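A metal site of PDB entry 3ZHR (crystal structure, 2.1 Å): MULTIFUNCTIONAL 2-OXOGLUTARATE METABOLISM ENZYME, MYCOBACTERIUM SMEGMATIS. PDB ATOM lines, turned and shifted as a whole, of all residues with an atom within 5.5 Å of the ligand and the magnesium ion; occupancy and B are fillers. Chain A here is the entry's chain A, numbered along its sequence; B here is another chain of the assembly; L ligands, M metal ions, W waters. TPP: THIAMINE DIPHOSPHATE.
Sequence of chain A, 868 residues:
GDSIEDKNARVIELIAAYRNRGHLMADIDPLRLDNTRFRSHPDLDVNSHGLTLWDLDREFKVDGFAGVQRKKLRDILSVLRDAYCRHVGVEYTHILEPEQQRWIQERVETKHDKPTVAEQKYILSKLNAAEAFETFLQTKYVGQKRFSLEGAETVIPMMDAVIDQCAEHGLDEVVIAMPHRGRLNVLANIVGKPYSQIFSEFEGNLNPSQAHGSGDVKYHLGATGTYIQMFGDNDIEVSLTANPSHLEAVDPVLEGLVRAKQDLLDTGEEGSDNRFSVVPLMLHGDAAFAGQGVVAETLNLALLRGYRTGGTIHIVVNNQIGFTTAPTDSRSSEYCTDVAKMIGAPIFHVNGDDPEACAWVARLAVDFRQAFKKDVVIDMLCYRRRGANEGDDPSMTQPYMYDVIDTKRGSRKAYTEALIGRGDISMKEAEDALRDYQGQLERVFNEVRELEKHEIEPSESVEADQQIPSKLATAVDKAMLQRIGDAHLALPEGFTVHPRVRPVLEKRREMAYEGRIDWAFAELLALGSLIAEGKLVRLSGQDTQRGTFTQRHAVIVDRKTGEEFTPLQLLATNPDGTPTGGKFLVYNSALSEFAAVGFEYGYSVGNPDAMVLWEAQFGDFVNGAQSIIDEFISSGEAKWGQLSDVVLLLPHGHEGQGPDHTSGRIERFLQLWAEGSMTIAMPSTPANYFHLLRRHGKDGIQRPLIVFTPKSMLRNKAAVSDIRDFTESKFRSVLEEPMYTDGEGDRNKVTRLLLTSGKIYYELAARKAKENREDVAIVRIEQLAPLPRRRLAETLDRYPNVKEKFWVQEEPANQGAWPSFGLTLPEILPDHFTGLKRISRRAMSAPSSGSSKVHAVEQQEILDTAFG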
ATOM      1  N   ARG A 181     -22.912   4.481 -13.661  1.00  0.00           N
ATOM      2  CA  ARG A 181     -22.709   5.700 -12.842  1.00  0.00           C
ATOM      3  C   ARG A 181     -23.876   5.999 -11.871  1.00  0.00           C
ATOM      4  O   ARG A 181     -24.953   6.394 -12.286  1.00  0.00           O
ATOM      5  CB  ARG A 181     -22.392   6.923 -13.708  1.00  0.00           C
ATOM      6  CG  ARG A 181     -21.561   7.968 -12.979  1.00  0.00           C
ATOM      7  CD  ARG A 181     -21.125   9.125 -13.877  1.00  0.00           C
ATOM      8  NE  ARG A 181     -20.151   8.711 -14.902  1.00  0.00           N
ATOM      9  CZ  ARG A 181     -18.878   8.429 -14.658  1.00  0.00           C
ATOM     10  NH1 ARG A 181     -18.393   8.526 -13.425  1.00  0.00           N
ATOM     11  NH2 ARG A 181     -18.069   8.098 -15.654  1.00  0.00           N
ATOM     12  N   SER A 245     -22.487  -3.997 -20.046  1.00  0.00           N
ATOM     13  CA  SER A 245     -21.672  -2.786 -20.017  1.00  0.00           C
ATOM     14  C   SER A 245     -21.867  -2.000 -21.324  1.00  0.00           C
ATOM     15  O   SER A 245     -21.508  -0.830 -21.352  1.00  0.00           O
ATOM     16  CB  SER A 245     -20.195  -3.099 -19.769  1.00  0.00           C
ATOM     17  OG  SER A 245     -19.966  -3.675 -18.502  1.00  0.00           O
ATOM     18  N   HIS A 246     -22.449  -2.627 -22.391  1.00  0.00           N
ATOM     19  CA  HIS A 246     -22.730  -1.969 -23.692  1.00  0.00           C
ATOM     20  C   HIS A 246     -23.711  -0.870 -23.464  1.00  0.00           C
ATOM     21  O   HIS A 246     -24.893  -1.148 -23.220  1.00  0.00           O
ATOM     22  CB  HIS A 246     -23.283  -2.970 -24.742  1.00  0.00           C
ATOM     23  CG  HIS A 246     -22.270  -3.983 -25.163  1.00  0.00           C
ATOM     24  ND1 HIS A 246     -21.577  -4.732 -24.238  1.00  0.00           N
ATOM     25  CD2 HIS A 246     -21.874  -4.344 -26.398  1.00  0.00           C
ATOM     26  CE1 HIS A 246     -20.742  -5.496 -24.932  1.00  0.00           C
ATOM     27  NE2 HIS A 246     -20.908  -5.316 -26.248  1.00  0.00           N
ATOM     28  N   LEU A 247     -23.198   0.383 -23.451  1.00  0.00           N
ATOM     29  CA  LEU A 247     -23.981   1.585 -23.171  1.00  0.00           C
ATOM     30  C   LEU A 247     -25.095   1.736 -24.170  1.00  0.00           C
ATOM     31  O   LEU A 247     -24.884   1.503 -25.359  1.00  0.00           O
ATOM     32  CB  LEU A 247     -23.077   2.836 -23.194  1.00  0.00           C
ATOM     33  CG  LEU A 247     -21.917   2.888 -22.145  1.00  0.00           C
ATOM     34  CD1 LEU A 247     -20.947   3.993 -22.447  1.00  0.00           C
ATOM     35  CD2 LEU A 247     -22.436   3.042 -20.722  1.00  0.00           C
ATOM     36  N   GLY A 285     -25.641   8.670 -20.491  1.00  0.00           N
ATOM     37  CA  GLY A 285     -24.454   9.511 -20.440  1.00  0.00           C
ATOM     38  C   GLY A 285     -24.468  10.353 -21.706  1.00  0.00           C
ATOM     39  O   GLY A 285     -25.058   9.934 -22.706  1.00  0.00           O
ATOM     40  N   ASP A 286     -23.842  11.539 -21.678  1.00  0.00           N
ATOM     41  CA  ASP A 286     -23.820  12.468 -22.810  1.00  0.00           C
ATOM     42  C   ASP A 286     -23.129  11.916 -24.047  1.00  0.00           C
ATOM     43  O   ASP A 286     -23.630  12.147 -25.144  1.00  0.00           O
ATOM     44  CB  ASP A 286     -23.161  13.812 -22.416  1.00  0.00           C
ATOM     45  CG  ASP A 286     -21.807  13.693 -21.728  1.00  0.00           C
ATOM     46  OD1 ASP A 286     -21.740  13.086 -20.636  1.00  0.00           O
ATOM     47  OD2 ASP A 286     -20.820  14.232 -22.276  1.00  0.00           O
ATOM     48  N   ALA A 287     -21.983  11.224 -23.898  1.00  0.00           N
ATOM     49  CA  ALA A 287     -21.281  10.743 -25.096  1.00  0.00           C
ATOM     50  C   ALA A 287     -22.028   9.577 -25.741  1.00  0.00           C
ATOM     51  O   ALA A 287     -22.156   9.551 -26.960  1.00  0.00           O
ATOM     52  CB  ALA A 287     -19.821  10.352 -24.783  1.00  0.00           C
ATOM     53  N   ALA A 288     -22.575   8.671 -24.942  1.00  0.00           N
ATOM     54  CA  ALA A 288     -23.291   7.493 -25.431  1.00  0.00           C
ATOM     55  C   ALA A 288     -24.622   7.869 -26.080  1.00  0.00           C
ATOM     56  O   ALA A 288     -24.988   7.257 -27.085  1.00  0.00           O
ATOM     57  CB  ALA A 288     -23.514   6.494 -24.303  1.00  0.00           C
ATOM     58  N   PHE A 289     -25.325   8.887 -25.539  1.00  0.00           N
ATOM     59  CA  PHE A 289     -26.618   9.344 -26.067  1.00  0.00           C
ATOM     60  C   PHE A 289     -26.484   9.888 -27.475  1.00  0.00           C
ATOM     61  O   PHE A 289     -27.378   9.688 -28.291  1.00  0.00           O
ATOM     62  CB  PHE A 289     -27.269  10.408 -25.132  1.00  0.00           C
ATOM     63  CG  PHE A 289     -28.751  10.581 -25.346  1.00  0.00           C
ATOM     64  CD1 PHE A 289     -29.659   9.583 -24.981  1.00  0.00           C
ATOM     65  CD2 PHE A 289     -29.262  11.754 -25.901  1.00  0.00           C
ATOM     66  CE1 PHE A 289     -31.036   9.769 -25.155  1.00  0.00           C
ATOM     67  CE2 PHE A 289     -30.633  11.927 -26.077  1.00  0.00           C
ATOM     68  CZ  PHE A 289     -31.514  10.947 -25.686  1.00  0.00           C
ATOM     69  N   GLN A 292     -24.535   6.467 -30.028  1.00  0.00           N
ATOM     70  CA  GLN A 292     -25.095   5.120 -30.220  1.00  0.00           C
ATOM     71  C   GLN A 292     -26.376   5.158 -31.061  1.00  0.00           C
ATOM     72  O   GLN A 292     -27.353   5.793 -30.683  1.00  0.00           O
ATOM     73  CB  GLN A 292     -25.303   4.430 -28.866  1.00  0.00           C
ATOM     74  CG  GLN A 292     -23.974   4.052 -28.147  1.00  0.00           C
ATOM     75  CD  GLN A 292     -23.276   2.893 -28.833  1.00  0.00           C
ATOM     76  OE1 GLN A 292     -23.873   1.839 -29.052  1.00  0.00           O
ATOM     77  NE2 GLN A 292     -22.008   3.037 -29.198  1.00  0.00           N
ATOM     78  N   VAL A 317     -27.178  12.247 -17.889  1.00  0.00           N
ATOM     79  CA  VAL A 317     -26.212  12.703 -16.897  1.00  0.00           C
ATOM     80  C   VAL A 317     -25.070  13.289 -17.753  1.00  0.00           C
ATOM     81  O   VAL A 317     -24.206  12.545 -18.244  1.00  0.00           O
ATOM     82  CB  VAL A 317     -25.780  11.574 -15.925  1.00  0.00           C
ATOM     83  CG1 VAL A 317     -24.710  12.055 -14.937  1.00  0.00           C
ATOM     84  CG2 VAL A 317     -27.001  11.031 -15.148  1.00  0.00           C
ATOM     85  N   ASN A 318     -25.161  14.609 -18.028  1.00  0.00           N
ATOM     86  CA  ASN A 318     -24.234  15.280 -18.920  1.00  0.00           C
ATOM     87  C   ASN A 318     -23.084  15.936 -18.156  1.00  0.00           C
ATOM     88  O   ASN A 318     -23.149  17.125 -17.847  1.00  0.00           O
ATOM     89  CB  ASN A 318     -25.006  16.305 -19.775  1.00  0.00           C
ATOM     90  CG  ASN A 318     -24.180  17.032 -20.801  1.00  0.00           C
ATOM     91  OD1 ASN A 318     -22.999  16.718 -21.032  1.00  0.00           O
ATOM     92  ND2 ASN A 318     -24.795  17.997 -21.461  1.00  0.00           N
ATOM     93  N   ASN A 319     -22.017  15.148 -17.905  1.00  0.00           N
ATOM     94  CA  ASN A 319     -20.820  15.603 -17.178  1.00  0.00           C
ATOM     95  C   ASN A 319     -19.765  16.186 -18.147  1.00  0.00           C
ATOM     96  O   ASN A 319     -18.616  16.447 -17.748  1.00  0.00           O
ATOM     97  CB  ASN A 319     -20.228  14.494 -16.329  1.00  0.00           C
ATOM     98  CG  ASN A 319     -19.994  13.184 -17.046  1.00  0.00           C
ATOM     99  OD1 ASN A 319     -19.851  13.150 -18.260  1.00  0.00           O
ATOM    100  ND2 ASN A 319     -19.942  12.085 -16.291  1.00  0.00           N
ATOM    101  N   GLN A 320     -20.176  16.382 -19.440  1.00  0.00           N
ATOM    102  CA  GLN A 320     -19.425  17.109 -20.494  1.00  0.00           C
ATOM    103  C   GLN A 320     -18.077  16.467 -20.806  1.00  0.00           C
ATOM    104  O   GLN A 320     -17.126  17.131 -21.235  1.00  0.00           O
ATOM    105  CB  GLN A 320     -19.242  18.602 -20.059  1.00  0.00           C
ATOM    106  CG  GLN A 320     -20.568  19.241 -19.573  1.00  0.00           C
ATOM    107  CD  GLN A 320     -20.383  20.631 -18.998  1.00  0.00           C
ATOM    108  OE1 GLN A 320     -20.063  21.577 -19.713  1.00  0.00           O
ATOM    109  NE2 GLN A 320     -20.607  20.805 -17.698  1.00  0.00           N
ATOM    110  N   ILE A 321     -18.022  15.139 -20.662  1.00  0.00           N
ATOM    111  CA  ILE A 321     -16.827  14.333 -20.925  1.00  0.00           C
ATOM    112  C   ILE A 321     -17.287  12.907 -21.183  1.00  0.00           C
ATOM    113  O   ILE A 321     -18.345  12.474 -20.672  1.00  0.00           O
ATOM    114  CB  ILE A 321     -15.775  14.445 -19.754  1.00  0.00           C
ATOM    115  CG1 ILE A 321     -14.369  13.885 -20.185  1.00  0.00           C
ATOM    116  CG2 ILE A 321     -16.297  13.822 -18.413  1.00  0.00           C
ATOM    117  CD1 ILE A 321     -13.212  14.234 -19.264  1.00  0.00           C
ATOM    118  N   GLY A 322     -16.527  12.236 -22.018  1.00  0.00           N
ATOM    119  CA  GLY A 322     -16.768  10.837 -22.360  1.00  0.00           C
ATOM    120  C   GLY A 322     -15.453  10.086 -22.234  1.00  0.00           C
ATOM    121  O   GLY A 322     -14.682  10.026 -23.208  1.00  0.00           O
ATOM    122  N   PHE A 323     -15.145   9.599 -21.010  1.00  0.00           N
ATOM    123  CA  PHE A 323     -13.902   8.882 -20.663  1.00  0.00           C
ATOM    124  C   PHE A 323     -12.740   9.912 -20.716  1.00  0.00           C
ATOM    125  O   PHE A 323     -12.543  10.647 -19.746  1.00  0.00           O
ATOM    126  CB  PHE A 323     -13.700   7.646 -21.596  1.00  0.00           C
ATOM    127  CG  PHE A 323     -12.864   6.506 -21.027  1.00  0.00           C
ATOM    128  CD1 PHE A 323     -13.439   5.512 -20.260  1.00  0.00           C
ATOM    129  CD2 PHE A 323     -11.492   6.474 -21.227  1.00  0.00           C
ATOM    130  CE1 PHE A 323     -12.666   4.467 -19.747  1.00  0.00           C
ATOM    131  CE2 PHE A 323     -10.706   5.440 -20.687  1.00  0.00           C
ATOM    132  CZ  PHE A 323     -11.307   4.452 -19.940  1.00  0.00           C
ATOM    133  N   ARG A 384     -17.847  15.375 -13.608  1.00  0.00           N
ATOM    134  CA  ARG A 384     -17.389  14.085 -13.136  1.00  0.00           C
ATOM    135  C   ARG A 384     -16.153  14.369 -12.282  1.00  0.00           C
ATOM    136  O   ARG A 384     -15.096  14.683 -12.840  1.00  0.00           O
ATOM    137  CB  ARG A 384     -17.090  13.201 -14.388  1.00  0.00           C
ATOM    138  CG  ARG A 384     -16.814  11.720 -14.136  1.00  0.00           C
ATOM    139  CD  ARG A 384     -16.064  11.103 -15.324  1.00  0.00           C
ATOM    140  NE  ARG A 384     -14.694  11.603 -15.377  1.00  0.00           N
ATOM    141  CZ  ARG A 384     -13.830  11.400 -16.365  1.00  0.00           C
ATOM    142  NH1 ARG A 384     -14.184  10.690 -17.435  1.00  0.00           N
ATOM    143  NH2 ARG A 384     -12.613  11.916 -16.312  1.00  0.00           N
ATOM    144  N   GLN B 542     -12.021   4.758 -29.590  1.00  0.00           N
ATOM    145  CA  GLN B 542     -12.457   5.442 -28.389  1.00  0.00           C
ATOM    146  C   GLN B 542     -11.269   5.653 -27.442  1.00  0.00           C
ATOM    147  O   GLN B 542     -10.570   4.686 -27.079  1.00  0.00           O
ATOM    148  CB  GLN B 542     -13.587   4.633 -27.727  1.00  0.00           C
ATOM    149  CG  GLN B 542     -14.952   4.835 -28.430  1.00  0.00           C
ATOM    150  CD  GLN B 542     -15.862   3.695 -28.186  1.00  0.00           C
ATOM    151  OE1 GLN B 542     -15.740   2.974 -27.179  1.00  0.00           O
ATOM    152  NE2 GLN B 542     -16.740   3.432 -29.136  1.00  0.00           N
ATOM    153  N   ASP B 543     -10.967   6.947 -27.165  1.00  0.00           N
ATOM    154  CA  ASP B 543      -9.881   7.367 -26.258  1.00  0.00           C
ATOM    155  C   ASP B 543      -8.494   6.864 -26.716  1.00  0.00           C
ATOM    156  O   ASP B 543      -7.581   6.710 -25.893  1.00  0.00           O
ATOM    157  CB  ASP B 543     -10.204   6.882 -24.834  1.00  0.00           C
ATOM    158  CG  ASP B 543     -11.594   7.344 -24.444  1.00  0.00           C
ATOM    159  OD1 ASP B 543     -11.780   8.588 -24.277  1.00  0.00           O
ATOM    160  OD2 ASP B 543     -12.512   6.494 -24.419  1.00  0.00           O
ATOM    161  N   LEU B 591     -18.560   7.978 -29.644  1.00  0.00           N
ATOM    162  CA  LEU B 591     -18.930   6.752 -28.952  1.00  0.00           C
ATOM    163  C   LEU B 591     -19.829   5.899 -29.843  1.00  0.00           C
ATOM    164  O   LEU B 591     -21.011   5.684 -29.533  1.00  0.00           O
ATOM    165  CB  LEU B 591     -19.612   7.028 -27.611  1.00  0.00           C
ATOM    166  CG  LEU B 591     -19.258   6.051 -26.502  1.00  0.00           C
ATOM    167  CD1 LEU B 591     -19.643   6.623 -25.161  1.00  0.00           C
ATOM    168  CD2 LEU B 591     -19.894   4.625 -26.725  1.00  0.00           C
ATOM    169  N   GLU B 593     -19.496   2.272 -32.664  1.00  0.00           N
ATOM    170  CA  GLU B 593     -18.700   1.159 -33.163  1.00  0.00           C
ATOM    171  C   GLU B 593     -19.078   0.958 -34.614  1.00  0.00           C
ATOM    172  O   GLU B 593     -18.213   1.022 -35.475  1.00  0.00           O
ATOM    173  CB  GLU B 593     -18.892  -0.128 -32.322  1.00  0.00           C
ATOM    174  CG  GLU B 593     -18.187  -0.065 -30.988  1.00  0.00           C
ATOM    175  CD  GLU B 593     -18.936   0.672 -29.879  1.00  0.00           C
ATOM    176  OE1 GLU B 593     -20.187   0.711 -29.916  1.00  0.00           O
ATOM    177  OE2 GLU B 593     -18.259   1.199 -28.977  1.00  0.00           O
ATOM    178  N   GLN B 617     -12.477  -0.066 -27.593  1.00  0.00           N
ATOM    179  CA  GLN B 617     -12.119   0.270 -26.220  1.00  0.00           C
ATOM    180  C   GLN B 617     -11.705  -1.039 -25.508  1.00  0.00           C
ATOM    181  O   GLN B 617     -10.661  -1.122 -24.826  1.00  0.00           O
ATOM    182  CB  GLN B 617     -13.266   1.018 -25.499  1.00  0.00           C
ATOM    183  CG  GLN B 617     -12.730   2.276 -24.871  1.00  0.00           C
ATOM    184  CD  GLN B 617     -13.239   2.591 -23.506  1.00  0.00           C
ATOM    185  OE1 GLN B 617     -13.670   1.728 -22.743  1.00  0.00           O
ATOM    186  NE2 GLN B 617     -13.146   3.831 -23.149  1.00  0.00           N
ATOM    187  N   PHE B 621     -16.892  -4.793 -27.386  1.00  0.00           N
ATOM    188  CA  PHE B 621     -17.819  -3.816 -27.932  1.00  0.00           C
ATOM    189  C   PHE B 621     -17.874  -3.825 -29.458  1.00  0.00           C
ATOM    190  O   PHE B 621     -18.773  -3.203 -30.020  1.00  0.00           O
ATOM    191  CB  PHE B 621     -17.498  -2.403 -27.405  1.00  0.00           C
ATOM    192  CG  PHE B 621     -17.556  -2.342 -25.902  1.00  0.00           C
ATOM    193  CD1 PHE B 621     -18.727  -2.661 -25.225  1.00  0.00           C
ATOM    194  CD2 PHE B 621     -16.437  -2.003 -25.166  1.00  0.00           C
ATOM    195  CE1 PHE B 621     -18.772  -2.650 -23.831  1.00  0.00           C
ATOM    196  CE2 PHE B 621     -16.476  -1.999 -23.760  1.00  0.00           C
ATOM    197  CZ  PHE B 621     -17.645  -2.315 -23.100  1.00  0.00           C
ATOM    198  N   HIS B 661     -15.684  -7.167 -20.676  1.00  0.00           N
ATOM    199  CA  HIS B 661     -14.321  -6.620 -20.626  1.00  0.00           C
ATOM    200  C   HIS B 661     -13.347  -7.805 -20.628  1.00  0.00           C
ATOM    201  O   HIS B 661     -12.319  -7.792 -19.959  1.00  0.00           O
ATOM    202  CB  HIS B 661     -14.147  -5.707 -19.412  1.00  0.00           C
ATOM    203  CG  HIS B 661     -15.071  -4.535 -19.424  1.00  0.00           C
ATOM    204  ND1 HIS B 661     -14.693  -3.317 -19.957  1.00  0.00           N
ATOM    205  CD2 HIS B 661     -16.362  -4.424 -18.991  1.00  0.00           C
ATOM    206  CE1 HIS B 661     -15.738  -2.518 -19.829  1.00  0.00           C
ATOM    207  NE2 HIS B 661     -16.770  -3.134 -19.272  1.00  0.00           N
HETATM  208  N1' TPP L   1     -19.038   1.202 -26.303  1.00  0.00           N
HETATM  209  C2' TPP L   1     -20.137   0.711 -25.738  1.00  0.00           C
HETATM  210  CM2 TPP L   1     -21.303   0.334 -26.599  1.00  0.00           C
HETATM  211  N3' TPP L   1     -20.204   0.556 -24.425  1.00  0.00           N
HETATM  212  C4' TPP L   1     -19.160   0.853 -23.636  1.00  0.00           C
HETATM  213  N4' TPP L   1     -19.263   0.577 -22.309  1.00  0.00           N
HETATM  214  C5' TPP L   1     -17.986   1.393 -24.188  1.00  0.00           C
HETATM  215  C6' TPP L   1     -17.971   1.525 -25.571  1.00  0.00           C
HETATM  216  C7' TPP L   1     -16.766   1.811 -23.388  1.00  0.00           C
HETATM  217  N3  TPP L   1     -17.008   2.997 -22.528  1.00  0.00           N
HETATM  218  C2  TPP L   1     -17.179   2.844 -21.247  1.00  0.00           C
HETATM  219  S1  TPP L   1     -17.379   4.349 -20.453  1.00  0.00           S
HETATM  220  C5  TPP L   1     -17.161   5.215 -21.979  1.00  0.00           C
HETATM  221  C4  TPP L   1     -17.002   4.270 -22.947  1.00  0.00           C
HETATM  222  CM4 TPP L   1     -16.736   4.753 -24.373  1.00  0.00           C
HETATM  223  C6  TPP L   1     -17.335   6.713 -22.107  1.00  0.00           C
HETATM  224  C7  TPP L   1     -18.800   6.994 -21.677  1.00  0.00           C
HETATM  225  O7  TPP L   1     -19.181   8.372 -21.803  1.00  0.00           O
HETATM  226  PA  TPP L   1     -20.612   8.897 -21.311  1.00  0.00           P
HETATM  227  O1A TPP L   1     -21.698   8.281 -22.159  1.00  0.00           O
HETATM  228  O2A TPP L   1     -20.657  10.486 -21.487  1.00  0.00           O
HETATM  229  O3A TPP L   1     -20.839   8.420 -19.783  1.00  0.00           O
HETATM  230  PB  TPP L   1     -20.064   8.799 -18.511  1.00  0.00           P
HETATM  231  O1B TPP L   1     -18.958   7.699 -18.201  1.00  0.00           O
HETATM  232  O2B TPP L   1     -19.440  10.135 -18.817  1.00  0.00           O
HETATM  233  O3B TPP L   1     -21.188   8.877 -17.374  1.00  0.00           O
HETATM  234 MG    MG M   1     -20.276  11.780 -19.842  1.00  0.00          MG
HETATM  235  O   HOH W   1     -16.602   7.105 -18.640  1.00  0.00           O
HETATM  236  O   HOH W   2     -14.916   7.595 -25.266  1.00  0.00           O
HETATM  237  O   HOH W   3     -16.668   9.957 -18.624  1.00  0.00           O
HETATM  238  O   HOH W   4     -23.159   6.393 -20.565  1.00  0.00           O
HETATM  239  O   HOH W   5     -23.151   7.272 -17.804  1.00  0.00           O
HETATM  240  O   HOH W   6     -20.762   5.501 -18.957  1.00  0.00           O
HETATM  241  O   HOH W   7     -20.989  -2.048 -29.143  1.00  0.00           O
HETATM  242  O   HOH W   8     -21.936  11.248 -18.726  1.00  0.00           O
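Water W8 is bound to the magnesium ion (2.1 Å).
The magnesium ion is bound by an oxygen (O2B) of the ligand, 2.1 Å away.
OD1 of Asp 286 binds the magnesium ion.
O2A of the ligand is bound to the magnesium ion.
The magnesium ion is bound by OD1 of Asn 319 (2.1 Å).
The backbone carbonyl oxygen (O) of Ile 321 is bound to the magnesium ion (2.2 Å).
The magnesium ion has six donor atoms within binding distance.
The side-chain amide nitrogen (NE2) of Gln 542 of chain B sits at hydrogen-bond distance from the side-chain carboxylate (OE2) of Glu 593 of chain B (2.7 Å).
The side-chain carboxylate of Glu 593 of chain B is in hydrogen-bond range of the side-chain amide nitrogen of Gln 292, at 3.0 Å.
The side-chain hydroxyl (OG) of Ser 245 sits at hydrogen-bond distance from a ring nitrogen (NE2) of His 661 of chain B (3.3 Å).
The side-chain amide nitrogen (NE2) of Gln 617 of chain B is in hydrogen-bond range of the side-chain carboxylate (OD2) of Asp 543 of chain B.
The backbone carbonyl oxygen (O) of Leu 591 of chain B sits at hydrogen-bond distance from the side-chain amide nitrogen (NE2) of Gln 292, at 2.8 Å.
O of Phe 323 is in hydrogen-bond range of NH1 of Arg 384 (2.8 Å).
Water W8 lies within hydrogen-bond range of the backbone carbonyl oxygen (O) of Val 317 (2.7 Å), an oxygen (O3B) of the ligand (2.8 Å) and the side-chain amide nitrogen (ND2) of Asn 319 (3.3 Å).
Water W1 lies within hydrogen-bond range of an oxygen (O1B) of the ligand and the guanidinium group of Arg 181.
Water W3 lies within hydrogen-bond range of NH1 of Arg 384, N of Phe 323 and O1B of the ligand.
Water W4 bridges an oxygen (O1A) of the ligand (2.9 Å) and the backbone NH of Gly 285 (3.4 Å).
Water W2 bridges the side-chain carboxylate (OD2) of Asp 543 of chain B (2.8 Å) and the backbone carbonyl oxygen (O) of Gly 322 (3.2 Å).
Water W7 bridges O of Phe 621 of chain B (2.6 Å) and OE1 of Glu 593 of chain B (3.0 Å).
The backbone NH (N) of Asp 286 sits close to an oxygen (O2A) of the ligand (3.4 Å).
O3B of the ligand lies within salt-bridge range of NE of Arg 181 (2.7 Å).
The side-chain carboxylate of Glu 593 of chain B is in hydrogen-bond range of a nitrogen (N1') of the ligand (2.8 Å).
The backbone carbonyl oxygen (O) of Ser 245 lies within hydrogen-bond range of a nitrogen (N4') of the ligand (2.8 Å).
An oxygen (O1A) of the ligand lies within hydrogen-bond range of the backbone NH (N) of Ala 287 (3.4 Å).
An oxygen (O1A) of the ligand sits at hydrogen-bond distance from the backbone NH (N) of Ala 288 (2.9 Å).
The backbone NH (N) of Leu 247 sits at hydrogen-bond distance from a nitrogen (N3') of the ligand (3.2 Å).
Within 4 Å of the magnesium ion: Asp 286, Asn 319 and Ile 321.
Along chain A the residues within 4 Å of the magnesium ion span positions 286 to 321.
The nearest printed residue that does not touch the magnesium ion is Val 317 (4.3 Å).
Merely in contact with the ligand: Gln 542 of chain B (3.1 Å), Gln 617 of chain B (3.2 Å), Phe 621 of chain B (3.4 Å), Gly 285 (3.5 Å), Gly 322 (3.5 Å), Leu 591 of chain B (3.5 Å), His 246 (3.6 Å), Phe 323 (3.8 Å) and Gln 292 (3.8 Å).
Hydrophobic or aromatic side chains within 4 Å of the ligand: Leu 247, Ala 287, Ala 288, Phe 323, Leu 591 of chain B and Phe 621 of chain B.
Within 4 Å of the ligand: Arg 181, Ser 245, His 246, Leu 247, Gly 285, Asp 286, Ala 287, Ala 288, Gln 292, Asn 319, Ile 321, Gly 322, Phe 323, Gln 542 of chain B, Leu 591 of chain B, Glu 593 of chain B, Gln 617 of chain B and Phe 621 of chain B.
The nearest printed residue that does not touch the ligand is Asp 543 of chain B (4.6 Å).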
